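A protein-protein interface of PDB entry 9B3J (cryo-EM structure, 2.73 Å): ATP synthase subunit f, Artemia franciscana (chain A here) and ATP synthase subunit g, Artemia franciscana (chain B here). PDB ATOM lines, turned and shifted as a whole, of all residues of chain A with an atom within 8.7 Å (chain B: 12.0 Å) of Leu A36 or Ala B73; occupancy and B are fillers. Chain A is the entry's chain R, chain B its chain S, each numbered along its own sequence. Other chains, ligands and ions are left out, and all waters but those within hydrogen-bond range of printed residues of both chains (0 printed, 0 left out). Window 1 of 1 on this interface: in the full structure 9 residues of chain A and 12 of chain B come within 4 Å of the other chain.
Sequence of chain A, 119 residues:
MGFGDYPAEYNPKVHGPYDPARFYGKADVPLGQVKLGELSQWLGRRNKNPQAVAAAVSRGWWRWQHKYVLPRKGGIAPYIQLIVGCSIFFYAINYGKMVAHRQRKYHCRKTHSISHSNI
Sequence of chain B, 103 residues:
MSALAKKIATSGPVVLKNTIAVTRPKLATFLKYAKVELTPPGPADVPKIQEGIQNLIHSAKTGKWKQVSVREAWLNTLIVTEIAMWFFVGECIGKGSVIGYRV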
ATOM      1  N   PRO A  30     -14.344  23.608 -21.502  1.00  0.00           N
ATOM      2  CA  PRO A  30     -15.197  23.181 -22.613  1.00  0.00           C
ATOM      3  C   PRO A  30     -16.185  22.120 -22.167  1.00  0.00           C
ATOM      4  O   PRO A  30     -15.915  21.333 -21.255  1.00  0.00           O
ATOM      5  CB  PRO A  30     -14.201  22.619 -23.630  1.00  0.00           C
ATOM      6  CG  PRO A  30     -13.045  22.190 -22.806  1.00  0.00           C
ATOM      7  CD  PRO A  30     -12.948  23.180 -21.687  1.00  0.00           C
ATOM      8  N   LEU A  31     -17.342  22.098 -22.835  1.00  0.00           N
ATOM      9  CA  LEU A  31     -18.444  21.245 -22.406  1.00  0.00           C
ATOM     10  C   LEU A  31     -18.133  19.767 -22.559  1.00  0.00           C
ATOM     11  O   LEU A  31     -18.810  18.949 -21.939  1.00  0.00           O
ATOM     12  CB  LEU A  31     -19.721  21.583 -23.181  1.00  0.00           C
ATOM     13  CG  LEU A  31     -20.013  20.898 -24.518  1.00  0.00           C
ATOM     14  CD1 LEU A  31     -21.444  21.167 -24.932  1.00  0.00           C
ATOM     15  CD2 LEU A  31     -19.063  21.357 -25.606  1.00  0.00           C
ATOM     16  N   GLY A  32     -17.129  19.411 -23.359  1.00  0.00           N
ATOM     17  CA  GLY A  32     -16.798  18.008 -23.531  1.00  0.00           C
ATOM     18  C   GLY A  32     -16.260  17.364 -22.270  1.00  0.00           C
ATOM     19  O   GLY A  32     -16.597  16.220 -21.957  1.00  0.00           O
ATOM     20  N   GLN A  33     -15.432  18.089 -21.518  1.00  0.00           N
ATOM     21  CA  GLN A  33     -14.747  17.527 -20.364  1.00  0.00           C
ATOM     22  C   GLN A  33     -15.373  17.938 -19.038  1.00  0.00           C
ATOM     23  O   GLN A  33     -14.747  17.754 -17.991  1.00  0.00           O
ATOM     24  CB  GLN A  33     -13.271  17.920 -20.388  1.00  0.00           C
ATOM     25  CG  GLN A  33     -13.032  19.414 -20.341  1.00  0.00           C
ATOM     26  CD  GLN A  33     -11.569  19.776 -20.493  1.00  0.00           C
ATOM     27  OE1 GLN A  33     -11.158  20.890 -20.170  1.00  0.00           O
ATOM     28  NE2 GLN A  33     -10.773  18.836 -20.991  1.00  0.00           N
ATOM     29  N   VAL A  34     -16.583  18.493 -19.056  1.00  0.00           N
ATOM     30  CA  VAL A  34     -17.287  18.788 -17.812  1.00  0.00           C
ATOM     31  C   VAL A  34     -17.775  17.485 -17.196  1.00  0.00           C
ATOM     32  O   VAL A  34     -18.426  16.673 -17.864  1.00  0.00           O
ATOM     33  CB  VAL A  34     -18.454  19.749 -18.070  1.00  0.00           C
ATOM     34  CG1 VAL A  34     -19.261  19.961 -16.802  1.00  0.00           C
ATOM     35  CG2 VAL A  34     -17.932  21.067 -18.588  1.00  0.00           C
ATOM     36  N   LYS A  35     -17.491  17.289 -15.907  1.00  0.00           N
ATOM     37  CA  LYS A  35     -17.728  16.007 -15.252  1.00  0.00           C
ATOM     38  C   LYS A  35     -19.198  15.749 -14.913  1.00  0.00           C
ATOM     39  O   LYS A  35     -19.476  14.764 -14.218  1.00  0.00           O
ATOM     40  CB  LYS A  35     -16.880  15.901 -13.983  1.00  0.00           C
ATOM     41  CG  LYS A  35     -17.332  16.800 -12.847  1.00  0.00           C
ATOM     42  CD  LYS A  35     -16.551  16.508 -11.575  1.00  0.00           C
ATOM     43  CE  LYS A  35     -17.099  17.299 -10.401  1.00  0.00           C
ATOM     44  NZ  LYS A  35     -18.520  16.949 -10.117  1.00  0.00           N
ATOM     45  N   LEU A  36     -20.115  16.628 -15.338  1.00  0.00           N
ATOM     46  CA  LEU A  36     -21.572  16.476 -15.271  1.00  0.00           C
ATOM     47  C   LEU A  36     -22.113  16.593 -13.847  1.00  0.00           C
ATOM     48  O   LEU A  36     -23.330  16.623 -13.642  1.00  0.00           O
ATOM     49  CB  LEU A  36     -22.024  15.156 -15.914  1.00  0.00           C
ATOM     50  CG  LEU A  36     -23.442  15.067 -16.486  1.00  0.00           C
ATOM     51  CD1 LEU A  36     -23.411  14.599 -17.926  1.00  0.00           C
ATOM     52  CD2 LEU A  36     -24.302  14.142 -15.647  1.00  0.00           C
ATOM     53  N   GLY A  37     -21.229  16.681 -12.857  1.00  0.00           N
ATOM     54  CA  GLY A  37     -21.641  17.017 -11.510  1.00  0.00           C
ATOM     55  C   GLY A  37     -21.635  18.520 -11.344  1.00  0.00           C
ATOM     56  O   GLY A  37     -22.268  19.067 -10.437  1.00  0.00           O
ATOM     57  N   GLU A  38     -20.913  19.195 -12.238  1.00  0.00           N
ATOM     58  CA  GLU A  38     -20.873  20.650 -12.291  1.00  0.00           C
ATOM     59  C   GLU A  38     -21.442  21.175 -13.601  1.00  0.00           C
ATOM     60  O   GLU A  38     -21.130  22.299 -14.003  1.00  0.00           O
ATOM     61  CB  GLU A  38     -19.443  21.153 -12.088  1.00  0.00           C
ATOM     62  CG  GLU A  38     -18.820  20.736 -10.763  1.00  0.00           C
ATOM     63  CD  GLU A  38     -19.405  21.475  -9.567  1.00  0.00           C
ATOM     64  OE1 GLU A  38     -19.875  22.619  -9.737  1.00  0.00           O
ATOM     65  OE2 GLU A  38     -19.391  20.908  -8.454  1.00  0.00           O
ATOM     66  N   LEU A  39     -22.269  20.372 -14.277  1.00  0.00           N
ATOM     67  CA  LEU A  39     -22.811  20.767 -15.573  1.00  0.00           C
ATOM     68  C   LEU A  39     -23.804  21.914 -15.440  1.00  0.00           C
ATOM     69  O   LEU A  39     -23.868  22.791 -16.310  1.00  0.00           O
ATOM     70  CB  LEU A  39     -23.467  19.567 -16.248  1.00  0.00           C
ATOM     71  CG  LEU A  39     -23.865  19.779 -17.705  1.00  0.00           C
ATOM     72  CD1 LEU A  39     -22.641  20.107 -18.537  1.00  0.00           C
ATOM     73  CD2 LEU A  39     -24.571  18.552 -18.244  1.00  0.00           C
ATOM     74  N   SER A  40     -24.599  21.919 -14.367  1.00  0.00           N
ATOM     75  CA  SER A  40     -25.511  23.032 -14.125  1.00  0.00           C
ATOM     76  C   SER A  40     -24.747  24.310 -13.803  1.00  0.00           C
ATOM     77  O   SER A  40     -25.155  25.405 -14.208  1.00  0.00           O
ATOM     78  CB  SER A  40     -26.478  22.682 -12.997  1.00  0.00           C
ATOM     79  OG  SER A  40     -25.772  22.364 -11.812  1.00  0.00           O
ATOM     80  N   GLN A  41     -23.631  24.186 -13.080  1.00  0.00           N
ATOM     81  CA  GLN A  41     -22.777  25.341 -12.820  1.00  0.00           C
ATOM     82  C   GLN A  41     -22.127  25.845 -14.102  1.00  0.00           C
ATOM     83  O   GLN A  41     -21.965  27.057 -14.287  1.00  0.00           O
ATOM     84  CB  GLN A  41     -21.709  24.985 -11.786  1.00  0.00           C
ATOM     85  CG  GLN A  41     -22.209  24.922 -10.348  1.00  0.00           C
ATOM     86  CD  GLN A  41     -22.992  23.658 -10.037  1.00  0.00           C
ATOM     87  OE1 GLN A  41     -23.065  22.738 -10.852  1.00  0.00           O
ATOM     88  NE2 GLN A  41     -23.585  23.610  -8.851  1.00  0.00           N
ATOM     89  N   TRP A  42     -21.742  24.928 -14.991  1.00  0.00           N
ATOM     90  CA  TRP A  42     -21.188  25.322 -16.281  1.00  0.00           C
ATOM     91  C   TRP A  42     -22.229  26.031 -17.137  1.00  0.00           C
ATOM     92  O   TRP A  42     -21.914  27.016 -17.813  1.00  0.00           O
ATOM     93  CB  TRP A  42     -20.639  24.094 -17.008  1.00  0.00           C
ATOM     94  CG  TRP A  42     -19.934  24.396 -18.294  1.00  0.00           C
ATOM     95  CD1 TRP A  42     -18.599  24.598 -18.465  1.00  0.00           C
ATOM     96  CD2 TRP A  42     -20.528  24.513 -19.594  1.00  0.00           C
ATOM     97  NE1 TRP A  42     -18.323  24.841 -19.788  1.00  0.00           N
ATOM     98  CE2 TRP A  42     -19.493  24.795 -20.500  1.00  0.00           C
ATOM     99  CE3 TRP A  42     -21.836  24.411 -20.076  1.00  0.00           C
ATOM    100  CZ2 TRP A  42     -19.722  24.975 -21.860  1.00  0.00           C
ATOM    101  CZ3 TRP A  42     -22.061  24.593 -21.425  1.00  0.00           C
ATOM    102  CH2 TRP A  42     -21.012  24.871 -22.301  1.00  0.00           C
ATOM    103  N   LEU B  56     -23.336  -1.161 -11.802  1.00  0.00           N
ATOM    104  CA  LEU B  56     -24.213  -0.097 -12.277  1.00  0.00           C
ATOM    105  C   LEU B  56     -25.239   0.266 -11.215  1.00  0.00           C
ATOM    106  O   LEU B  56     -25.585   1.444 -11.052  1.00  0.00           O
ATOM    107  CB  LEU B  56     -24.901  -0.516 -13.578  1.00  0.00           C
ATOM    108  CG  LEU B  56     -24.268  -0.109 -14.911  1.00  0.00           C
ATOM    109  CD1 LEU B  56     -24.130   1.397 -14.997  1.00  0.00           C
ATOM    110  CD2 LEU B  56     -22.926  -0.778 -15.130  1.00  0.00           C
ATOM    111  N   SER B  59     -23.491   2.250  -9.095  1.00  0.00           N
ATOM    112  CA  SER B  59     -23.448   3.570  -9.702  1.00  0.00           C
ATOM    113  C   SER B  59     -24.821   4.224  -9.779  1.00  0.00           C
ATOM    114  O   SER B  59     -24.913   5.390 -10.173  1.00  0.00           O
ATOM    115  CB  SER B  59     -22.845   3.488 -11.106  1.00  0.00           C
ATOM    116  OG  SER B  59     -21.570   2.873 -11.076  1.00  0.00           O
ATOM    117  N   THR B  62     -24.816   5.547  -5.314  1.00  0.00           N
ATOM    118  CA  THR B  62     -23.743   6.286  -4.665  1.00  0.00           C
ATOM    119  C   THR B  62     -23.161   7.383  -5.546  1.00  0.00           C
ATOM    120  O   THR B  62     -23.115   8.546  -5.138  1.00  0.00           O
ATOM    121  CB  THR B  62     -22.632   5.319  -4.241  1.00  0.00           C
ATOM    122  OG1 THR B  62     -22.077   4.691  -5.402  1.00  0.00           O
ATOM    123  CG2 THR B  62     -23.187   4.250  -3.317  1.00  0.00           C
ATOM    124  N   GLY B  63     -22.720   7.036  -6.750  1.00  0.00           N
ATOM    125  CA  GLY B  63     -22.060   7.995  -7.613  1.00  0.00           C
ATOM    126  C   GLY B  63     -21.676   7.408  -8.953  1.00  0.00           C
ATOM    127  O   GLY B  63     -22.502   6.773  -9.615  1.00  0.00           O
ATOM    128  N   LYS B  64     -20.432   7.656  -9.374  1.00  0.00           N
ATOM    129  CA  LYS B  64     -19.836   7.153 -10.617  1.00  0.00           C
ATOM    130  C   LYS B  64     -20.566   7.635 -11.867  1.00  0.00           C
ATOM    131  O   LYS B  64     -20.365   7.081 -12.952  1.00  0.00           O
ATOM    132  CB  LYS B  64     -19.745   5.619 -10.628  1.00  0.00           C
ATOM    133  CG  LYS B  64     -19.115   5.011  -9.387  1.00  0.00           C
ATOM    134  CD  LYS B  64     -17.650   5.374  -9.265  1.00  0.00           C
ATOM    135  CE  LYS B  64     -17.063   4.808  -7.985  1.00  0.00           C
ATOM    136  NZ  LYS B  64     -17.286   3.339  -7.877  1.00  0.00           N
ATOM    137  N   TRP B  65     -21.416   8.651 -11.741  1.00  0.00           N
ATOM    138  CA  TRP B  65     -22.071   9.268 -12.883  1.00  0.00           C
ATOM    139  C   TRP B  65     -22.026  10.786 -12.855  1.00  0.00           C
ATOM    140  O   TRP B  65     -22.147  11.405 -13.918  1.00  0.00           O
ATOM    141  CB  TRP B  65     -23.533   8.811 -12.982  1.00  0.00           C
ATOM    142  CG  TRP B  65     -24.431   9.502 -12.021  1.00  0.00           C
ATOM    143  CD1 TRP B  65     -24.381   9.438 -10.660  1.00  0.00           C
ATOM    144  CD2 TRP B  65     -25.525  10.362 -12.345  1.00  0.00           C
ATOM    145  NE1 TRP B  65     -25.376  10.212 -10.115  1.00  0.00           N
ATOM    146  CE2 TRP B  65     -26.094  10.789 -11.130  1.00  0.00           C
ATOM    147  CE3 TRP B  65     -26.079  10.815 -13.545  1.00  0.00           C
ATOM    148  CZ2 TRP B  65     -27.190  11.648 -11.080  1.00  0.00           C
ATOM    149  CZ3 TRP B  65     -27.168  11.666 -13.494  1.00  0.00           C
ATOM    150  CH2 TRP B  65     -27.710  12.074 -12.271  1.00  0.00           C
ATOM    151  N   LYS B  66     -21.850  11.403 -11.690  1.00  0.00           N
ATOM    152  CA  LYS B  66     -21.593  12.831 -11.580  1.00  0.00           C
ATOM    153  C   LYS B  66     -20.106  13.129 -11.623  1.00  0.00           C
ATOM    154  O   LYS B  66     -19.692  14.267 -11.371  1.00  0.00           O
ATOM    155  CB  LYS B  66     -22.224  13.378 -10.303  1.00  0.00           C
ATOM    156  CG  LYS B  66     -23.741  13.300 -10.314  1.00  0.00           C
ATOM    157  CD  LYS B  66     -24.323  13.624  -8.954  1.00  0.00           C
ATOM    158  CE  LYS B  66     -23.891  12.600  -7.919  1.00  0.00           C
ATOM    159  NZ  LYS B  66     -24.448  12.898  -6.570  1.00  0.00           N
ATOM    160  N   GLN B  67     -19.315  12.105 -11.935  1.00  0.00           N
ATOM    161  CA  GLN B  67     -17.888  12.143 -12.199  1.00  0.00           C
ATOM    162  C   GLN B  67     -17.619  11.699 -13.629  1.00  0.00           C
ATOM    163  O   GLN B  67     -16.596  11.065 -13.889  1.00  0.00           O
ATOM    164  CB  GLN B  67     -17.123  11.223 -11.247  1.00  0.00           C
ATOM    165  CG  GLN B  67     -16.975  11.707  -9.827  1.00  0.00           C
ATOM    166  CD  GLN B  67     -18.064  11.197  -8.911  1.00  0.00           C
ATOM    167  OE1 GLN B  67     -18.908  10.391  -9.306  1.00  0.00           O
ATOM    168  NE2 GLN B  67     -18.050  11.667  -7.674  1.00  0.00           N
ATOM    169  N   VAL B  68     -18.559  11.982 -14.544  1.00  0.00           N
ATOM    170  CA  VAL B  68     -18.534  11.518 -15.940  1.00  0.00           C
ATOM    171  C   VAL B  68     -18.436  12.723 -16.887  1.00  0.00           C
ATOM    172  O   VAL B  68     -19.393  13.502 -17.004  1.00  0.00           O
ATOM    173  CB  VAL B  68     -19.786  10.680 -16.264  1.00  0.00           C
ATOM    174  CG1 VAL B  68     -20.065  10.639 -17.720  1.00  0.00           C
ATOM    175  CG2 VAL B  68     -19.667   9.260 -15.738  1.00  0.00           C
ATOM    176  N   SER B  69     -17.312  12.838 -17.610  1.00  0.00           N
ATOM    177  CA  SER B  69     -17.114  13.897 -18.609  1.00  0.00           C
ATOM    178  C   SER B  69     -18.254  13.902 -19.618  1.00  0.00           C
ATOM    179  O   SER B  69     -18.694  12.832 -20.022  1.00  0.00           O
ATOM    180  CB  SER B  69     -15.817  13.641 -19.365  1.00  0.00           C
ATOM    181  OG  SER B  69     -16.073  12.766 -20.449  1.00  0.00           O
ATOM    182  N   VAL B  70     -18.730  15.080 -20.064  1.00  0.00           N
ATOM    183  CA  VAL B  70     -19.890  15.036 -20.973  1.00  0.00           C
ATOM    184  C   VAL B  70     -19.559  14.331 -22.283  1.00  0.00           C
ATOM    185  O   VAL B  70     -20.450  13.757 -22.901  1.00  0.00           O
ATOM    186  CB  VAL B  70     -20.510  16.419 -21.269  1.00  0.00           C
ATOM    187  CG1 VAL B  70     -21.679  16.333 -22.273  1.00  0.00           C
ATOM    188  CG2 VAL B  70     -21.039  17.045 -20.023  1.00  0.00           C
ATOM    189  N   ARG B  71     -18.294  14.323 -22.723  1.00  0.00           N
ATOM    190  CA  ARG B  71     -17.968  13.548 -23.921  1.00  0.00           C
ATOM    191  C   ARG B  71     -18.250  12.080 -23.665  1.00  0.00           C
ATOM    192  O   ARG B  71     -19.024  11.445 -24.393  1.00  0.00           O
ATOM    193  CB  ARG B  71     -16.502  13.755 -24.349  1.00  0.00           C
ATOM    194  CG  ARG B  71     -16.350  14.088 -25.851  1.00  0.00           C
ATOM    195  CD  ARG B  71     -14.931  14.151 -26.445  1.00  0.00           C
ATOM    196  NE  ARG B  71     -14.992  14.477 -27.872  1.00  0.00           N
ATOM    197  CZ  ARG B  71     -14.495  13.726 -28.847  1.00  0.00           C
ATOM    198  NH1 ARG B  71     -13.839  12.612 -28.591  1.00  0.00           N
ATOM    199  NH2 ARG B  71     -14.644  14.114 -30.111  1.00  0.00           N
ATOM    200  N   GLU B  72     -17.702  11.566 -22.565  1.00  0.00           N
ATOM    201  CA  GLU B  72     -17.974  10.198 -22.163  1.00  0.00           C
ATOM    202  C   GLU B  72     -19.460   9.989 -21.942  1.00  0.00           C
ATOM    203  O   GLU B  72     -20.024   9.065 -22.514  1.00  0.00           O
ATOM    204  CB  GLU B  72     -17.169   9.850 -20.920  1.00  0.00           C
ATOM    205  CG  GLU B  72     -17.638   8.666 -20.145  1.00  0.00           C
ATOM    206  CD  GLU B  72     -16.929   8.616 -18.826  1.00  0.00           C
ATOM    207  OE1 GLU B  72     -15.708   8.419 -18.802  1.00  0.00           O
ATOM    208  OE2 GLU B  72     -17.562   8.823 -17.811  1.00  0.00           O
ATOM    209  N   ALA B  73     -20.125  10.887 -21.202  1.00  0.00           N
ATOM    210  CA  ALA B  73     -21.568  10.746 -20.983  1.00  0.00           C
ATOM    211  C   ALA B  73     -22.341  10.747 -22.286  1.00  0.00           C
ATOM    212  O   ALA B  73     -23.268   9.945 -22.457  1.00  0.00           O
ATOM    213  CB  ALA B  73     -22.111  11.864 -20.102  1.00  0.00           C
ATOM    214  N   TRP B  74     -21.970  11.640 -23.207  1.00  0.00           N
ATOM    215  CA  TRP B  74     -22.568  11.699 -24.528  1.00  0.00           C
ATOM    216  C   TRP B  74     -22.543  10.350 -25.162  1.00  0.00           C
ATOM    217  O   TRP B  74     -23.581   9.796 -25.522  1.00  0.00           O
ATOM    218  CB  TRP B  74     -21.808  12.635 -25.456  1.00  0.00           C
ATOM    219  CG  TRP B  74     -22.390  12.730 -26.832  1.00  0.00           C
ATOM    220  CD1 TRP B  74     -21.708  12.781 -28.006  1.00  0.00           C
ATOM    221  CD2 TRP B  74     -23.774  12.848 -27.169  1.00  0.00           C
ATOM    222  NE1 TRP B  74     -22.579  12.927 -29.052  1.00  0.00           N
ATOM    223  CE2 TRP B  74     -23.853  12.967 -28.559  1.00  0.00           C
ATOM    224  CE3 TRP B  74     -24.957  12.882 -26.427  1.00  0.00           C
ATOM    225  CZ2 TRP B  74     -25.060  13.102 -29.217  1.00  0.00           C
ATOM    226  CZ3 TRP B  74     -26.132  13.007 -27.068  1.00  0.00           C
ATOM    227  CH2 TRP B  74     -26.189  13.116 -28.452  1.00  0.00           C
ATOM    228  N   LEU B  75     -21.331   9.792 -25.207  1.00  0.00           N
ATOM    229  CA  LEU B  75     -21.059   8.477 -25.767  1.00  0.00           C
ATOM    230  C   LEU B  75     -21.822   7.371 -25.060  1.00  0.00           C
ATOM    231  O   LEU B  75     -22.310   6.451 -25.718  1.00  0.00           O
ATOM    232  CB  LEU B  75     -19.569   8.169 -25.680  1.00  0.00           C
ATOM    233  CG  LEU B  75     -19.266   6.737 -26.109  1.00  0.00           C
ATOM    234  CD1 LEU B  75     -19.861   6.486 -27.485  1.00  0.00           C
ATOM    235  CD2 LEU B  75     -17.809   6.466 -26.174  1.00  0.00           C
ATOM    236  N   ASN B  76     -21.835   7.362 -23.728  1.00  0.00           N
ATOM    237  CA  ASN B  76     -22.549   6.286 -23.054  1.00  0.00           C
ATOM    238  C   ASN B  76     -24.005   6.302 -23.504  1.00  0.00           C
ATOM    239  O   ASN B  76     -24.502   5.282 -23.997  1.00  0.00           O
ATOM    240  CB  ASN B  76     -22.391   6.363 -21.524  1.00  0.00           C
ATOM    241  CG  ASN B  76     -21.071   5.729 -21.014  1.00  0.00           C
ATOM    242  OD1 ASN B  76     -20.052   5.751 -21.696  1.00  0.00           O
ATOM    243  ND2 ASN B  76     -21.101   5.175 -19.807  1.00  0.00           N
ATOM    244  N   THR B  77     -24.624   7.496 -23.543  1.00  0.00           N
ATOM    245  CA  THR B  77     -25.976   7.620 -24.103  1.00  0.00           C
ATOM    246  C   THR B  77     -26.046   7.126 -25.527  1.00  0.00           C
ATOM    247  O   THR B  77     -26.983   6.407 -25.896  1.00  0.00           O
ATOM    248  CB  THR B  77     -26.460   9.058 -24.089  1.00  0.00           C
ATOM    249  OG1 THR B  77     -27.026   9.281 -22.814  1.00  0.00           O
ATOM    250  CG2 THR B  77     -27.578   9.307 -25.129  1.00  0.00           C
ATOM    251  N   LEU B  78     -25.081   7.534 -26.343  1.00  0.00           N
ATOM    252  CA  LEU B  78     -25.063   7.134 -27.738  1.00  0.00           C
ATOM    253  C   LEU B  78     -25.097   5.624 -27.873  1.00  0.00           C
ATOM    254  O   LEU B  78     -25.981   5.075 -28.552  1.00  0.00           O
ATOM    255  CB  LEU B  78     -23.826   7.706 -28.413  1.00  0.00           C
ATOM    256  CG  LEU B  78     -24.153   8.922 -29.259  1.00  0.00           C
ATOM    257  CD1 LEU B  78     -23.160   9.118 -30.297  1.00  0.00           C
ATOM    258  CD2 LEU B  78     -25.512   8.772 -29.894  1.00  0.00           C
ATOM    259  N   ILE B  79     -24.171   4.947 -27.174  1.00  0.00           N
ATOM    260  CA  ILE B  79     -24.112   3.485 -27.128  1.00  0.00           C
ATOM    261  C   ILE B  79     -25.479   2.921 -26.806  1.00  0.00           C
ATOM    262  O   ILE B  79     -26.009   2.085 -27.544  1.00  0.00           O
ATOM    263  CB  ILE B  79     -23.092   2.997 -26.081  1.00  0.00           C
ATOM    264  CG1 ILE B  79     -21.653   3.141 -26.551  1.00  0.00           C
ATOM    265  CG2 ILE B  79     -23.382   1.535 -25.738  1.00  0.00           C
ATOM    266  CD1 ILE B  79     -21.268   2.106 -27.494  1.00  0.00           C
ATOM    267  N   VAL B  80     -26.102   3.424 -25.731  1.00  0.00           N
ATOM    268  CA  VAL B  80     -27.398   2.881 -25.321  1.00  0.00           C
ATOM    269  C   VAL B  80     -28.428   3.003 -26.438  1.00  0.00           C
ATOM    270  O   VAL B  80     -29.047   2.000 -26.802  1.00  0.00           O
ATOM    271  CB  VAL B  80     -27.885   3.518 -24.013  1.00  0.00           C
ATOM    272  CG1 VAL B  80     -29.403   3.598 -23.973  1.00  0.00           C
ATOM    273  CG2 VAL B  80     -27.409   2.657 -22.878  1.00  0.00           C
ATOM    274  N   THR B  81     -28.549   4.188 -27.061  1.00  0.00           N
ATOM    275  CA  THR B  81     -29.403   4.374 -28.242  1.00  0.00           C
ATOM    276  C   THR B  81     -29.161   3.303 -29.297  1.00  0.00           C
ATOM    277  O   THR B  81     -30.097   2.871 -29.979  1.00  0.00           O
ATOM    278  CB  THR B  81     -29.146   5.749 -28.861  1.00  0.00           C
ATOM    279  OG1 THR B  81     -28.899   6.699 -27.821  1.00  0.00           O
ATOM    280  CG2 THR B  81     -30.331   6.205 -29.673  1.00  0.00           C
ATOM    281  N   GLU B  82     -27.914   2.839 -29.412  1.00  0.00           N
ATOM    282  CA  GLU B  82     -27.618   1.732 -30.325  1.00  0.00           C
ATOM    283  C   GLU B  82     -28.274   0.434 -29.867  1.00  0.00           C
ATOM    284  O   GLU B  82     -28.781  -0.335 -30.693  1.00  0.00           O
ATOM    285  CB  GLU B  82     -26.109   1.551 -30.471  1.00  0.00           C
ATOM    286  CG  GLU B  82     -25.682   0.412 -31.330  1.00  0.00           C
ATOM    287  CD  GLU B  82     -24.180   0.275 -31.384  1.00  0.00           C
ATOM    288  OE1 GLU B  82     -23.484   1.312 -31.393  1.00  0.00           O
ATOM    289  OE2 GLU B  82     -23.693  -0.872 -31.411  1.00  0.00           O
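The backbone carbonyl oxygen (O) of Gly A32 is in hydrogen-bond range of the backbone NH (N) of Val B70 (3.1 Å). N of Arg B71 sits at hydrogen-bond distance from O of Gly A32 (2.7 Å). O of Val A34 is in hydrogen-bond range of N of Val B70. The side-chain amino group of Lys A35 lies within hydrogen-bond range of the backbone carbonyl oxygen of Lys B66, at 3.2 Å. The backbone carbonyl oxygen (O) of Lys A35 is in hydrogen-bond range of the backbone NH (N) of Val B68. The backbone NH (N) of Gly A37 lies within hydrogen-bond range of the backbone carbonyl oxygen (O) of Lys B66 (3.2 Å). The backbone carbonyl oxygen (O) of Val A34 lies close to the backbone carbonyl oxygen (O) of Val B68 (3.4 Å).
The side-chain amide oxygen (OE1) of Gln B67 lies within hydrogen-bond range of the backbone NH (N) of Lys B64, at 3.1 Å. The side-chain hydroxyl of Ser B69 is in hydrogen-bond range of the backbone NH of Glu B72 (2.9 Å).
Among the printed residues, merely in contact across the chains: Leu A31 with Val B70 (3.1 Å), Val A34 with Ser B69 (3.2 Å), Leu A36 with Val B68 (3.3 Å), Lys A35 with Gln B67 (3.5 Å), Gly A32 with Ser B69 (3.7 Å), Leu A36 with Ala B73 (3.7 Å), Leu A39 with Val B70 (3.8 Å), Leu A36 with Trp B65 (3.9 Å) and Lys A35 with Ser B69 (3.97 Å).
Printed residues of chain B within 4 Å of Leu A36: Trp B65, Val B68 and Ala B73. Gly A37 touches just one residue of chain B: Lys B66. No residue of chain B comes within 4 Å of Glu A38. Of chain B, only Val B70 comes within 4 Å of Leu A39. Trp A42 touches none of the printed residues of chain B. Of the printed residues of chain A, Val B68 touches Val A34 (3.4 Å), Lys A35 (2.9 Å) and Leu A36 (3.3 Å). Printed residues of chain A within 4 Å of Val B70: Leu A31, Gly A32, Val A34 and Leu A39. Of the printed residues of chain A, Arg B71 touches Gly A32. Ala B73 touches just one residue of chain A: Leu A36. Trp B74 touches none of the printed residues of chain A. The nearest printed residue of chain B that does not touch Leu A36 is Val B70 (4.001 Å). The nearest printed residue of chain A that does not touch Ala B73 is Gly A32 (6.4 Å).
Of the 23 printed residues of chain B, 8 touch a printed residue of chain A. Hydrophobic or aromatic side chains of chain B within 4 Å of the printed part of chain A: Val B70 and Ala B73. Among the printed residues, 16 pairs touch across the chains. Among the printed residues, no Asp or Glu carboxylate lies within 4 Å of a Lys or Arg side-chain nitrogen of the other chain.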
